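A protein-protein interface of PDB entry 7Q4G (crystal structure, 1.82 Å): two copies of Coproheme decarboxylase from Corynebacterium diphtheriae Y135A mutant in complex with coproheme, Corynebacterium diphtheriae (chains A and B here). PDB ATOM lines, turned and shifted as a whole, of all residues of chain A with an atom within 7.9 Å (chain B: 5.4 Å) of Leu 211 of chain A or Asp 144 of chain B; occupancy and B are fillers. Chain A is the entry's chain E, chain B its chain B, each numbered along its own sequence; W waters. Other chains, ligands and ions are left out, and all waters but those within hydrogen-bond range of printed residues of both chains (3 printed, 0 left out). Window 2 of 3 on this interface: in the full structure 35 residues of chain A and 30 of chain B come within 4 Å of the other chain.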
ATOM      1  N   ARG A 141     -18.223 -28.672  -3.244  1.00  0.00           N
ATOM      2  CA  ARG A 141     -19.336 -27.739  -3.288  1.00  0.00           C
ATOM      3  C   ARG A 141     -19.082 -26.597  -4.278  1.00  0.00           C
ATOM      4  O   ARG A 141     -17.942 -26.300  -4.646  1.00  0.00           O
ATOM      5  CB  ARG A 141     -19.562 -27.175  -1.893  1.00  0.00           C
ATOM      6  CG  ARG A 141     -20.180 -28.171  -0.976  1.00  0.00           C
ATOM      7  CD  ARG A 141     -21.669 -28.290  -1.223  1.00  0.00           C
ATOM      8  NE  ARG A 141     -22.336 -29.197  -0.316  1.00  0.00           N
ATOM      9  CZ  ARG A 141     -23.441 -29.839  -0.623  1.00  0.00           C
ATOM     10  NH1 ARG A 141     -24.047 -29.635  -1.784  1.00  0.00           N
ATOM     11  NH2 ARG A 141     -23.977 -30.655   0.265  1.00  0.00           N
ATOM     12  N   SER A 142     -20.176 -25.922  -4.674  1.00  0.00           N
ATOM     13  CA  SER A 142     -20.045 -24.710  -5.470  1.00  0.00           C
ATOM     14  C   SER A 142     -19.171 -23.692  -4.741  1.00  0.00           C
ATOM     15  O   SER A 142     -18.959 -23.766  -3.556  1.00  0.00           O
ATOM     16  CB  SER A 142     -21.437 -24.128  -5.761  1.00  0.00           C
ATOM     17  OG  SER A 142     -22.186 -23.928  -4.545  1.00  0.00           O
ATOM     18  N   ASP A 144     -19.864 -20.597  -4.134  1.00  0.00           N
ATOM     19  CA  ASP A 144     -20.686 -19.733  -3.289  1.00  0.00           C
ATOM     20  C   ASP A 144     -21.204 -20.410  -2.006  1.00  0.00           C
ATOM     21  O   ASP A 144     -21.850 -19.731  -1.202  1.00  0.00           O
ATOM     22  CB  ASP A 144     -21.873 -19.236  -4.134  1.00  0.00           C
ATOM     23  CG  ASP A 144     -22.966 -20.287  -4.344  1.00  0.00           C
ATOM     24  OD1 ASP A 144     -22.823 -21.449  -3.947  1.00  0.00           O
ATOM     25  OD2 ASP A 144     -24.016 -19.941  -4.946  1.00  0.00           O
ATOM     26  N   TRP A 145     -20.912 -21.688  -1.789  1.00  0.00           N
ATOM     27  CA  TRP A 145     -21.638 -22.455  -0.790  1.00  0.00           C
ATOM     28  C   TRP A 145     -21.321 -21.985   0.629  1.00  0.00           C
ATOM     29  O   TRP A 145     -22.213 -21.825   1.477  1.00  0.00           O
ATOM     30  CB  TRP A 145     -21.306 -23.931  -0.971  1.00  0.00           C
ATOM     31  CG  TRP A 145     -21.773 -24.859   0.103  1.00  0.00           C
ATOM     32  CD1 TRP A 145     -20.995 -25.575   0.961  1.00  0.00           C
ATOM     33  CD2 TRP A 145     -23.119 -25.223   0.371  1.00  0.00           C
ATOM     34  NE1 TRP A 145     -21.792 -26.365   1.769  1.00  0.00           N
ATOM     35  CE2 TRP A 145     -23.097 -26.174   1.408  1.00  0.00           C
ATOM     36  CE3 TRP A 145     -24.352 -24.865  -0.198  1.00  0.00           C
ATOM     37  CZ2 TRP A 145     -24.238 -26.751   1.905  1.00  0.00           C
ATOM     38  CZ3 TRP A 145     -25.503 -25.433   0.288  1.00  0.00           C
ATOM     39  CH2 TRP A 145     -25.449 -26.374   1.359  1.00  0.00           C
ATOM     40  N   MET A 148     -22.419 -18.451   1.549  1.00  0.00           N
ATOM     41  CA  MET A 148     -23.859 -18.297   1.707  1.00  0.00           C
ATOM     42  C   MET A 148     -24.200 -17.906   3.127  1.00  0.00           C
ATOM     43  O   MET A 148     -23.465 -18.231   4.075  1.00  0.00           O
ATOM     44  CB  MET A 148     -24.543 -19.653   1.365  1.00  0.00           C
ATOM     45  CG  MET A 148     -26.051 -19.648   1.427  1.00  0.00           C
ATOM     46  SD  MET A 148     -26.781 -21.286   0.879  1.00  0.00           S
ATOM     47  CE  MET A 148     -26.083 -21.447  -0.736  1.00  0.00           C
ATOM     48  N   LYS A 152     -29.285 -19.966   5.916  1.00  0.00           N
ATOM     49  CA  LYS A 152     -29.730 -20.495   4.636  1.00  0.00           C
ATOM     50  C   LYS A 152     -29.048 -21.826   4.355  1.00  0.00           C
ATOM     51  O   LYS A 152     -29.698 -22.803   3.971  1.00  0.00           O
ATOM     52  CB  LYS A 152     -29.467 -19.486   3.523  1.00  0.00           C
ATOM     53  CG  LYS A 152     -29.940 -19.934   2.136  1.00  0.00           C
ATOM     54  CD  LYS A 152     -29.511 -18.939   1.040  1.00  0.00           C
ATOM     55  CE  LYS A 152     -29.317 -19.630  -0.331  1.00  0.00           C
ATOM     56  NZ  LYS A 152     -30.363 -19.225  -1.342  1.00  0.00           N
ATOM     57  N   ILE A 156     -30.791 -25.499   4.240  1.00  0.00           N
ATOM     58  CA  ILE A 156     -30.613 -26.382   3.075  1.00  0.00           C
ATOM     59  C   ILE A 156     -30.120 -27.753   3.530  1.00  0.00           C
ATOM     60  O   ILE A 156     -30.685 -28.793   3.157  1.00  0.00           O
ATOM     61  CB  ILE A 156     -29.672 -25.722   2.048  1.00  0.00           C
ATOM     62  CG1 ILE A 156     -30.380 -24.564   1.364  1.00  0.00           C
ATOM     63  CG2 ILE A 156     -29.203 -26.759   0.987  1.00  0.00           C
ATOM     64  CD1 ILE A 156     -29.475 -23.635   0.481  1.00  0.00           C
ATOM     65  N   ARG A 205     -31.370 -36.414  -4.847  1.00  0.00           N
ATOM     66  CA  ARG A 205     -31.305 -35.430  -5.934  1.00  0.00           C
ATOM     67  C   ARG A 205     -32.434 -34.422  -5.830  1.00  0.00           C
ATOM     68  O   ARG A 205     -32.350 -33.338  -6.421  1.00  0.00           O
ATOM     69  CB  ARG A 205     -31.390 -36.148  -7.318  1.00  0.00           C
ATOM     70  CG  ARG A 205     -30.129 -36.894  -7.680  1.00  0.00           C
ATOM     71  CD  ARG A 205     -29.008 -35.887  -7.942  1.00  0.00           C
ATOM     72  NE  ARG A 205     -27.954 -36.453  -8.777  1.00  0.00           N
ATOM     73  CZ  ARG A 205     -26.931 -37.166  -8.341  1.00  0.00           C
ATOM     74  NH1 ARG A 205     -26.795 -37.472  -7.068  1.00  0.00           N
ATOM     75  NH2 ARG A 205     -25.989 -37.550  -9.205  1.00  0.00           N
ATOM     76  N   THR A 207     -33.389 -32.137  -3.820  1.00  0.00           N
ATOM     77  CA  THR A 207     -33.019 -31.264  -2.709  1.00  0.00           C
ATOM     78  C   THR A 207     -32.402 -29.974  -3.246  1.00  0.00           C
ATOM     79  O   THR A 207     -31.729 -29.958  -4.296  1.00  0.00           O
ATOM     80  CB  THR A 207     -32.011 -31.968  -1.747  1.00  0.00           C
ATOM     81  OG1 THR A 207     -30.858 -32.421  -2.503  1.00  0.00           O
ATOM     82  CG2 THR A 207     -32.692 -33.178  -1.048  1.00  0.00           C
ATOM     83  N   GLU A 208     -32.646 -28.897  -2.520  1.00  0.00           N
ATOM     84  CA  GLU A 208     -32.073 -27.606  -2.879  1.00  0.00           C
ATOM     85  C   GLU A 208     -30.553 -27.622  -2.825  1.00  0.00           C
ATOM     86  O   GLU A 208     -29.916 -26.876  -3.559  1.00  0.00           O
ATOM     87  CB  GLU A 208     -32.607 -26.501  -1.945  1.00  0.00           C
ATOM     88  CG  GLU A 208     -31.925 -25.136  -2.173  1.00  0.00           C
ATOM     89  CD  GLU A 208     -32.705 -23.973  -1.595  1.00  0.00           C
ATOM     90  OE1 GLU A 208     -33.476 -24.182  -0.635  1.00  0.00           O
ATOM     91  OE2 GLU A 208     -32.530 -22.845  -2.097  1.00  0.00           O
ATOM     92  N   ALA A 209     -29.960 -28.444  -1.950  1.00  0.00           N
ATOM     93  CA  ALA A 209     -28.516 -28.553  -1.851  1.00  0.00           C
ATOM     94  C   ALA A 209     -27.881 -28.878  -3.215  1.00  0.00           C
ATOM     95  O   ALA A 209     -26.719 -28.529  -3.449  1.00  0.00           O
ATOM     96  CB  ALA A 209     -28.116 -29.642  -0.839  1.00  0.00           C
ATOM     97  N   ARG A 210     -28.614 -29.541  -4.120  1.00  0.00           N
ATOM     98  CA  ARG A 210     -28.043 -29.913  -5.426  1.00  0.00           C
ATOM     99  C   ARG A 210     -27.749 -28.704  -6.297  1.00  0.00           C
ATOM    100  O   ARG A 210     -27.014 -28.826  -7.271  1.00  0.00           O
ATOM    101  CB  ARG A 210     -29.005 -30.831  -6.177  1.00  0.00           C
ATOM    102  CG  ARG A 210     -29.230 -32.194  -5.514  1.00  0.00           C
ATOM    103  CD  ARG A 210     -27.975 -33.000  -5.420  1.00  0.00           C
ATOM    104  NE  ARG A 210     -27.387 -33.211  -6.751  1.00  0.00           N
ATOM    105  CZ  ARG A 210     -26.199 -33.754  -6.962  1.00  0.00           C
ATOM    106  NH1 ARG A 210     -25.430 -34.161  -5.954  1.00  0.00           N
ATOM    107  NH2 ARG A 210     -25.744 -33.866  -8.208  1.00  0.00           N
ATOM    108  N   LEU A 211     -28.318 -27.538  -5.966  1.00  0.00           N
ATOM    109  CA  LEU A 211     -27.973 -26.293  -6.672  1.00  0.00           C
ATOM    110  C   LEU A 211     -26.650 -25.751  -6.250  1.00  0.00           C
ATOM    111  O   LEU A 211     -26.283 -24.625  -6.681  1.00  0.00           O
ATOM    112  CB  LEU A 211     -29.080 -25.255  -6.452  1.00  0.00           C
ATOM    113  CG  LEU A 211     -30.471 -25.783  -6.867  1.00  0.00           C
ATOM    114  CD1 LEU A 211     -31.487 -24.664  -6.758  1.00  0.00           C
ATOM    115  CD2 LEU A 211     -30.446 -26.322  -8.319  1.00  0.00           C
ATOM    116  N   HIS A 212     -25.877 -26.479  -5.437  1.00  0.00           N
ATOM    117  CA  HIS A 212     -24.636 -25.934  -4.907  1.00  0.00           C
ATOM    118  C   HIS A 212     -23.571 -26.994  -4.917  1.00  0.00           C
ATOM    119  O   HIS A 212     -22.892 -27.232  -3.928  1.00  0.00           O
ATOM    120  CB  HIS A 212     -24.864 -25.351  -3.499  1.00  0.00           C
ATOM    121  CG  HIS A 212     -25.859 -24.219  -3.474  1.00  0.00           C
ATOM    122  ND1 HIS A 212     -25.517 -22.915  -3.734  1.00  0.00           N
ATOM    123  CD2 HIS A 212     -27.196 -24.221  -3.312  1.00  0.00           C
ATOM    124  CE1 HIS A 212     -26.595 -22.156  -3.701  1.00  0.00           C
ATOM    125  NE2 HIS A 212     -27.628 -22.932  -3.475  1.00  0.00           N
ATOM    126  N   VAL A 213     -23.372 -27.593  -6.090  1.00  0.00           N
ATOM    127  CA  VAL A 213     -22.449 -28.726  -6.283  1.00  0.00           C
ATOM    128  C   VAL A 213     -21.558 -28.443  -7.463  1.00  0.00           C
ATOM    129  O   VAL A 213     -22.039 -27.897  -8.483  1.00  0.00           O
ATOM    130  CB  VAL A 213     -23.247 -30.049  -6.534  1.00  0.00           C
ATOM    131  CG1 VAL A 213     -22.310 -31.264  -6.670  1.00  0.00           C
ATOM    132  CG2 VAL A 213     -24.255 -30.240  -5.459  1.00  0.00           C
ATOM    133  N   ARG A 214     -20.276 -28.841  -7.343  1.00  0.00           N
ATOM    134  CA  ARG A 214     -19.347 -28.692  -8.469  1.00  0.00           C
ATOM    135  C   ARG A 214     -18.762 -30.004  -8.962  1.00  0.00           C
ATOM    136  O   ARG A 214     -18.490 -30.132 -10.168  1.00  0.00           O
ATOM    137  CB  ARG A 214     -18.148 -27.763  -8.107  1.00  0.00           C
ATOM    138  CG  ARG A 214     -18.248 -26.379  -8.548  1.00  0.00           C
ATOM    139  CD  ARG A 214     -16.871 -25.681  -8.503  1.00  0.00           C
ATOM    140  NE  ARG A 214     -16.304 -25.570  -7.169  1.00  0.00           N
ATOM    141  CZ  ARG A 214     -15.030 -25.765  -6.874  1.00  0.00           C
ATOM    142  NH1 ARG A 214     -14.148 -26.111  -7.793  1.00  0.00           N
ATOM    143  NH2 ARG A 214     -14.615 -25.599  -5.624  1.00  0.00           N
ATOM    144  N   SER B 142     -29.035 -31.882 -15.600  1.00  0.00           N
ATOM    145  CA  SER B 142     -28.624 -30.629 -14.958  1.00  0.00           C
ATOM    146  C   SER B 142     -28.870 -30.682 -13.437  1.00  0.00           C
ATOM    147  O   SER B 142     -29.659 -31.464 -12.915  1.00  0.00           O
ATOM    148  CB  SER B 142     -29.362 -29.464 -15.566  1.00  0.00           C
ATOM    149  OG  SER B 142     -30.735 -29.651 -15.544  1.00  0.00           O
ATOM    150  N   TYR B 143     -28.173 -29.805 -12.708  1.00  0.00           N
ATOM    151  CA  TYR B 143     -28.292 -29.841 -11.243  1.00  0.00           C
ATOM    152  C   TYR B 143     -29.702 -29.493 -10.797  1.00  0.00           C
ATOM    153  O   TYR B 143     -30.185 -29.990  -9.756  1.00  0.00           O
ATOM    154  CB  TYR B 143     -27.304 -28.855 -10.640  1.00  0.00           C
ATOM    155  CG  TYR B 143     -25.863 -29.291 -10.686  1.00  0.00           C
ATOM    156  CD1 TYR B 143     -25.443 -30.417  -9.948  1.00  0.00           C
ATOM    157  CD2 TYR B 143     -24.911 -28.608 -11.422  1.00  0.00           C
ATOM    158  CE1 TYR B 143     -24.148 -30.832  -9.964  1.00  0.00           C
ATOM    159  CE2 TYR B 143     -23.598 -29.024 -11.437  1.00  0.00           C
ATOM    160  CZ  TYR B 143     -23.211 -30.090 -10.717  1.00  0.00           C
ATOM    161  OH  TYR B 143     -21.897 -30.505 -10.713  1.00  0.00           O
ATOM    162  N   ASP B 144     -30.397 -28.657 -11.573  1.00  0.00           N
ATOM    163  CA  ASP B 144     -31.744 -28.180 -11.170  1.00  0.00           C
ATOM    164  C   ASP B 144     -32.873 -29.173 -11.515  1.00  0.00           C
ATOM    165  O   ASP B 144     -34.026 -28.905 -11.177  1.00  0.00           O
ATOM    166  CB  ASP B 144     -31.985 -26.840 -11.851  1.00  0.00           C
ATOM    167  CG  ASP B 144     -32.290 -26.990 -13.332  1.00  0.00           C
ATOM    168  OD1 ASP B 144     -32.107 -28.097 -13.884  1.00  0.00           O
ATOM    169  OD2 ASP B 144     -32.652 -25.973 -13.968  1.00  0.00           O
ATOM    170  N   TRP B 145     -32.556 -30.299 -12.122  1.00  0.00           N
ATOM    171  CA  TRP B 145     -33.593 -31.100 -12.805  1.00  0.00           C
ATOM    172  C   TRP B 145     -34.584 -31.707 -11.820  1.00  0.00           C
ATOM    173  O   TRP B 145     -35.802 -31.646 -12.056  1.00  0.00           O
ATOM    174  CB  TRP B 145     -32.927 -32.183 -13.655  1.00  0.00           C
ATOM    175  CG  TRP B 145     -33.855 -33.165 -14.294  1.00  0.00           C
ATOM    176  CD1 TRP B 145     -33.963 -34.518 -13.983  1.00  0.00           C
ATOM    177  CD2 TRP B 145     -34.797 -32.916 -15.330  1.00  0.00           C
ATOM    178  NE1 TRP B 145     -34.899 -35.114 -14.819  1.00  0.00           N
ATOM    179  CE2 TRP B 145     -35.443 -34.144 -15.628  1.00  0.00           C
ATOM    180  CE3 TRP B 145     -35.159 -31.770 -16.068  1.00  0.00           C
ATOM    181  CZ2 TRP B 145     -36.418 -34.252 -16.635  1.00  0.00           C
ATOM    182  CZ3 TRP B 145     -36.118 -31.878 -17.036  1.00  0.00           C
ATOM    183  CH2 TRP B 145     -36.755 -33.152 -17.306  1.00  0.00           C
ATOM    184  N   TYR B 146     -34.096 -32.248 -10.709  1.00  0.00           N
ATOM    185  CA  TYR B 146     -34.946 -33.025  -9.790  1.00  0.00           C
ATOM    186  C   TYR B 146     -35.624 -32.154  -8.762  1.00  0.00           C
ATOM    187  O   TYR B 146     -36.715 -32.512  -8.282  1.00  0.00           O
ATOM    188  CB  TYR B 146     -34.136 -34.086  -9.068  1.00  0.00           C
ATOM    189  CG  TYR B 146     -33.362 -34.997 -10.053  1.00  0.00           C
ATOM    190  CD1 TYR B 146     -32.084 -34.678 -10.484  1.00  0.00           C
ATOM    191  CD2 TYR B 146     -33.939 -36.131 -10.535  1.00  0.00           C
ATOM    192  CE1 TYR B 146     -31.380 -35.462 -11.330  1.00  0.00           C
ATOM    193  CE2 TYR B 146     -33.256 -36.977 -11.445  1.00  0.00           C
ATOM    194  CZ  TYR B 146     -31.987 -36.637 -11.833  1.00  0.00           C
ATOM    195  OH  TYR B 146     -31.317 -37.475 -12.705  1.00  0.00           O
ATOM    196  N   ILE B 147     -35.001 -31.006  -8.385  1.00  0.00           N
ATOM    197  CA  ILE B 147     -35.635 -30.099  -7.408  1.00  0.00           C
ATOM    198  C   ILE B 147     -36.609 -29.165  -8.099  1.00  0.00           C
ATOM    199  O   ILE B 147     -37.374 -28.476  -7.427  1.00  0.00           O
ATOM    200  CB  ILE B 147     -34.538 -29.334  -6.641  1.00  0.00           C
ATOM    201  CG1 ILE B 147     -35.130 -28.559  -5.430  1.00  0.00           C
ATOM    202  CG2 ILE B 147     -33.786 -28.446  -7.558  1.00  0.00           C
ATOM    203  CD1 ILE B 147     -35.950 -29.382  -4.471  1.00  0.00           C
ATOM    204  N   MET B 148     -36.608 -29.142  -9.433  1.00  0.00           N
ATOM    205  CA  MET B 148     -37.571 -28.367 -10.176  1.00  0.00           C
ATOM    206  C   MET B 148     -38.987 -28.753  -9.787  1.00  0.00           C
ATOM    207  O   MET B 148     -39.266 -29.919  -9.446  1.00  0.00           O
ATOM    208  CB  MET B 148     -37.334 -28.589 -11.671  1.00  0.00           C
ATOM    209  CG  MET B 148     -38.546 -28.445 -12.600  1.00  0.00           C
ATOM    210  SD  MET B 148     -38.099 -28.764 -14.361  1.00  0.00           S
ATOM    211  CE  MET B 148     -36.498 -28.082 -14.521  1.00  0.00           C
ATOM    212  N   HIS B 212     -31.702 -29.112 -19.851  1.00  0.00           N
ATOM    213  CA  HIS B 212     -31.456 -29.649 -18.508  1.00  0.00           C
ATOM    214  C   HIS B 212     -30.569 -30.887 -18.579  1.00  0.00           C
ATOM    215  O   HIS B 212     -30.882 -31.915 -17.975  1.00  0.00           O
ATOM    216  CB  HIS B 212     -32.817 -29.954 -17.872  1.00  0.00           C
ATOM    217  CG  HIS B 212     -33.665 -28.718 -17.692  1.00  0.00           C
ATOM    218  ND1 HIS B 212     -33.431 -27.806 -16.705  1.00  0.00           N
ATOM    219  CD2 HIS B 212     -34.677 -28.205 -18.429  1.00  0.00           C
ATOM    220  CE1 HIS B 212     -34.300 -26.809 -16.790  1.00  0.00           C
ATOM    221  NE2 HIS B 212     -35.073 -27.026 -17.829  1.00  0.00           N
HETATM  222  O   HOH W   1     -19.783 -28.762 -12.388  1.00  0.00           O
HETATM  223  O   HOH W   2     -28.905 -32.656  -9.140  1.00  0.00           O
HETATM  224  O   HOH W   3     -32.083 -31.525  -8.557  1.00  0.00           O
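Among the printed residues, pairs that only touch across the chains: Arg 205 of chain A with Tyr 146 of chain B (3.3 Å), Thr 207 of chain A with Ile 147 of chain B (3.7 Å), Glu 208 of chain A with Ile 147 of chain B (3.8 Å), Arg 210 of chain A with Tyr 143 of chain B (3.4 Å), Leu 211 of chain A with Tyr 143 of chain B (3.9 Å) and Leu 211 of chain A with Asp 144 of chain B (3.6 Å).
NE of Arg 214 of chain A lies within hydrogen-bond range of O of Arg 141 of chain A (3.1 Å). OD1 of Asp 144 of chain B lies within hydrogen-bond range of OG of Ser 142 of chain B, at 2.7 Å. OD1 of Asp 144 of chain B lies within hydrogen-bond range of ND1 of His 212 of chain B.
The backbone carbonyl oxygen (O) of Arg 214 of chain A sits at hydrogen-bond distance from the side-chain hydroxyl (OH) of Tyr 143 of chain B, 3.5 Å away. The backbone carbonyl oxygen (O) of Val 213 of chain A sits close to the side-chain hydroxyl (OH) of Tyr 143 of chain B (3.4 Å).
Positions printed for both chains: 142, 144, 145, 148 and 212.
Water W3 lies within hydrogen-bond range of the backbone carbonyl oxygen of Tyr 143 of chain B, the backbone carbonyl oxygen of Arg 205 of chain A, the backbone NH of Ile 147 of chain B and the backbone NH of Tyr 146 of chain B. Water W2 bridges the guanidinium group of Arg 210 of chain A (2.9 Å) and the backbone carbonyl oxygen of Tyr 143 of chain B (3.0 Å). Water W1 lies within hydrogen-bond range of O of Arg 214 of chain A and OH of Tyr 143 of chain B.
Hydrophobic or aromatic side chains of chain A within 4 Å of the printed part of chain B: Leu 211 and Val 213. Of the 8 printed residues of chain B, 4 touch a printed residue of chain A. Hydrophobic or aromatic side chains of chain B within 4 Å of the printed part of chain A: Tyr 143, Tyr 146 and Ile 147. Among the printed residues, no Asp or Glu carboxylate lies within 4 Å of a Lys or Arg side-chain nitrogen of the other chain.
Leu 211 of chain A touches just these residues of chain B: Tyr 143 and Asp 144. Of chain A, only Leu 211 comes within 4 Å of Asp 144 of chain B. Of the printed residues of chain B, Val 213 of chain A touches Tyr 143 (3.3 Å). Printed residues of chain B within 4 Å of Arg 214 of chain A: Tyr 143 (3.5 Å). Of the printed residues of chain B, Arg 210 of chain A touches Tyr 143. The nearest printed residue of chain B that does not touch Arg 210 of chain A is Asp 144 of chain B (5.5 Å).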
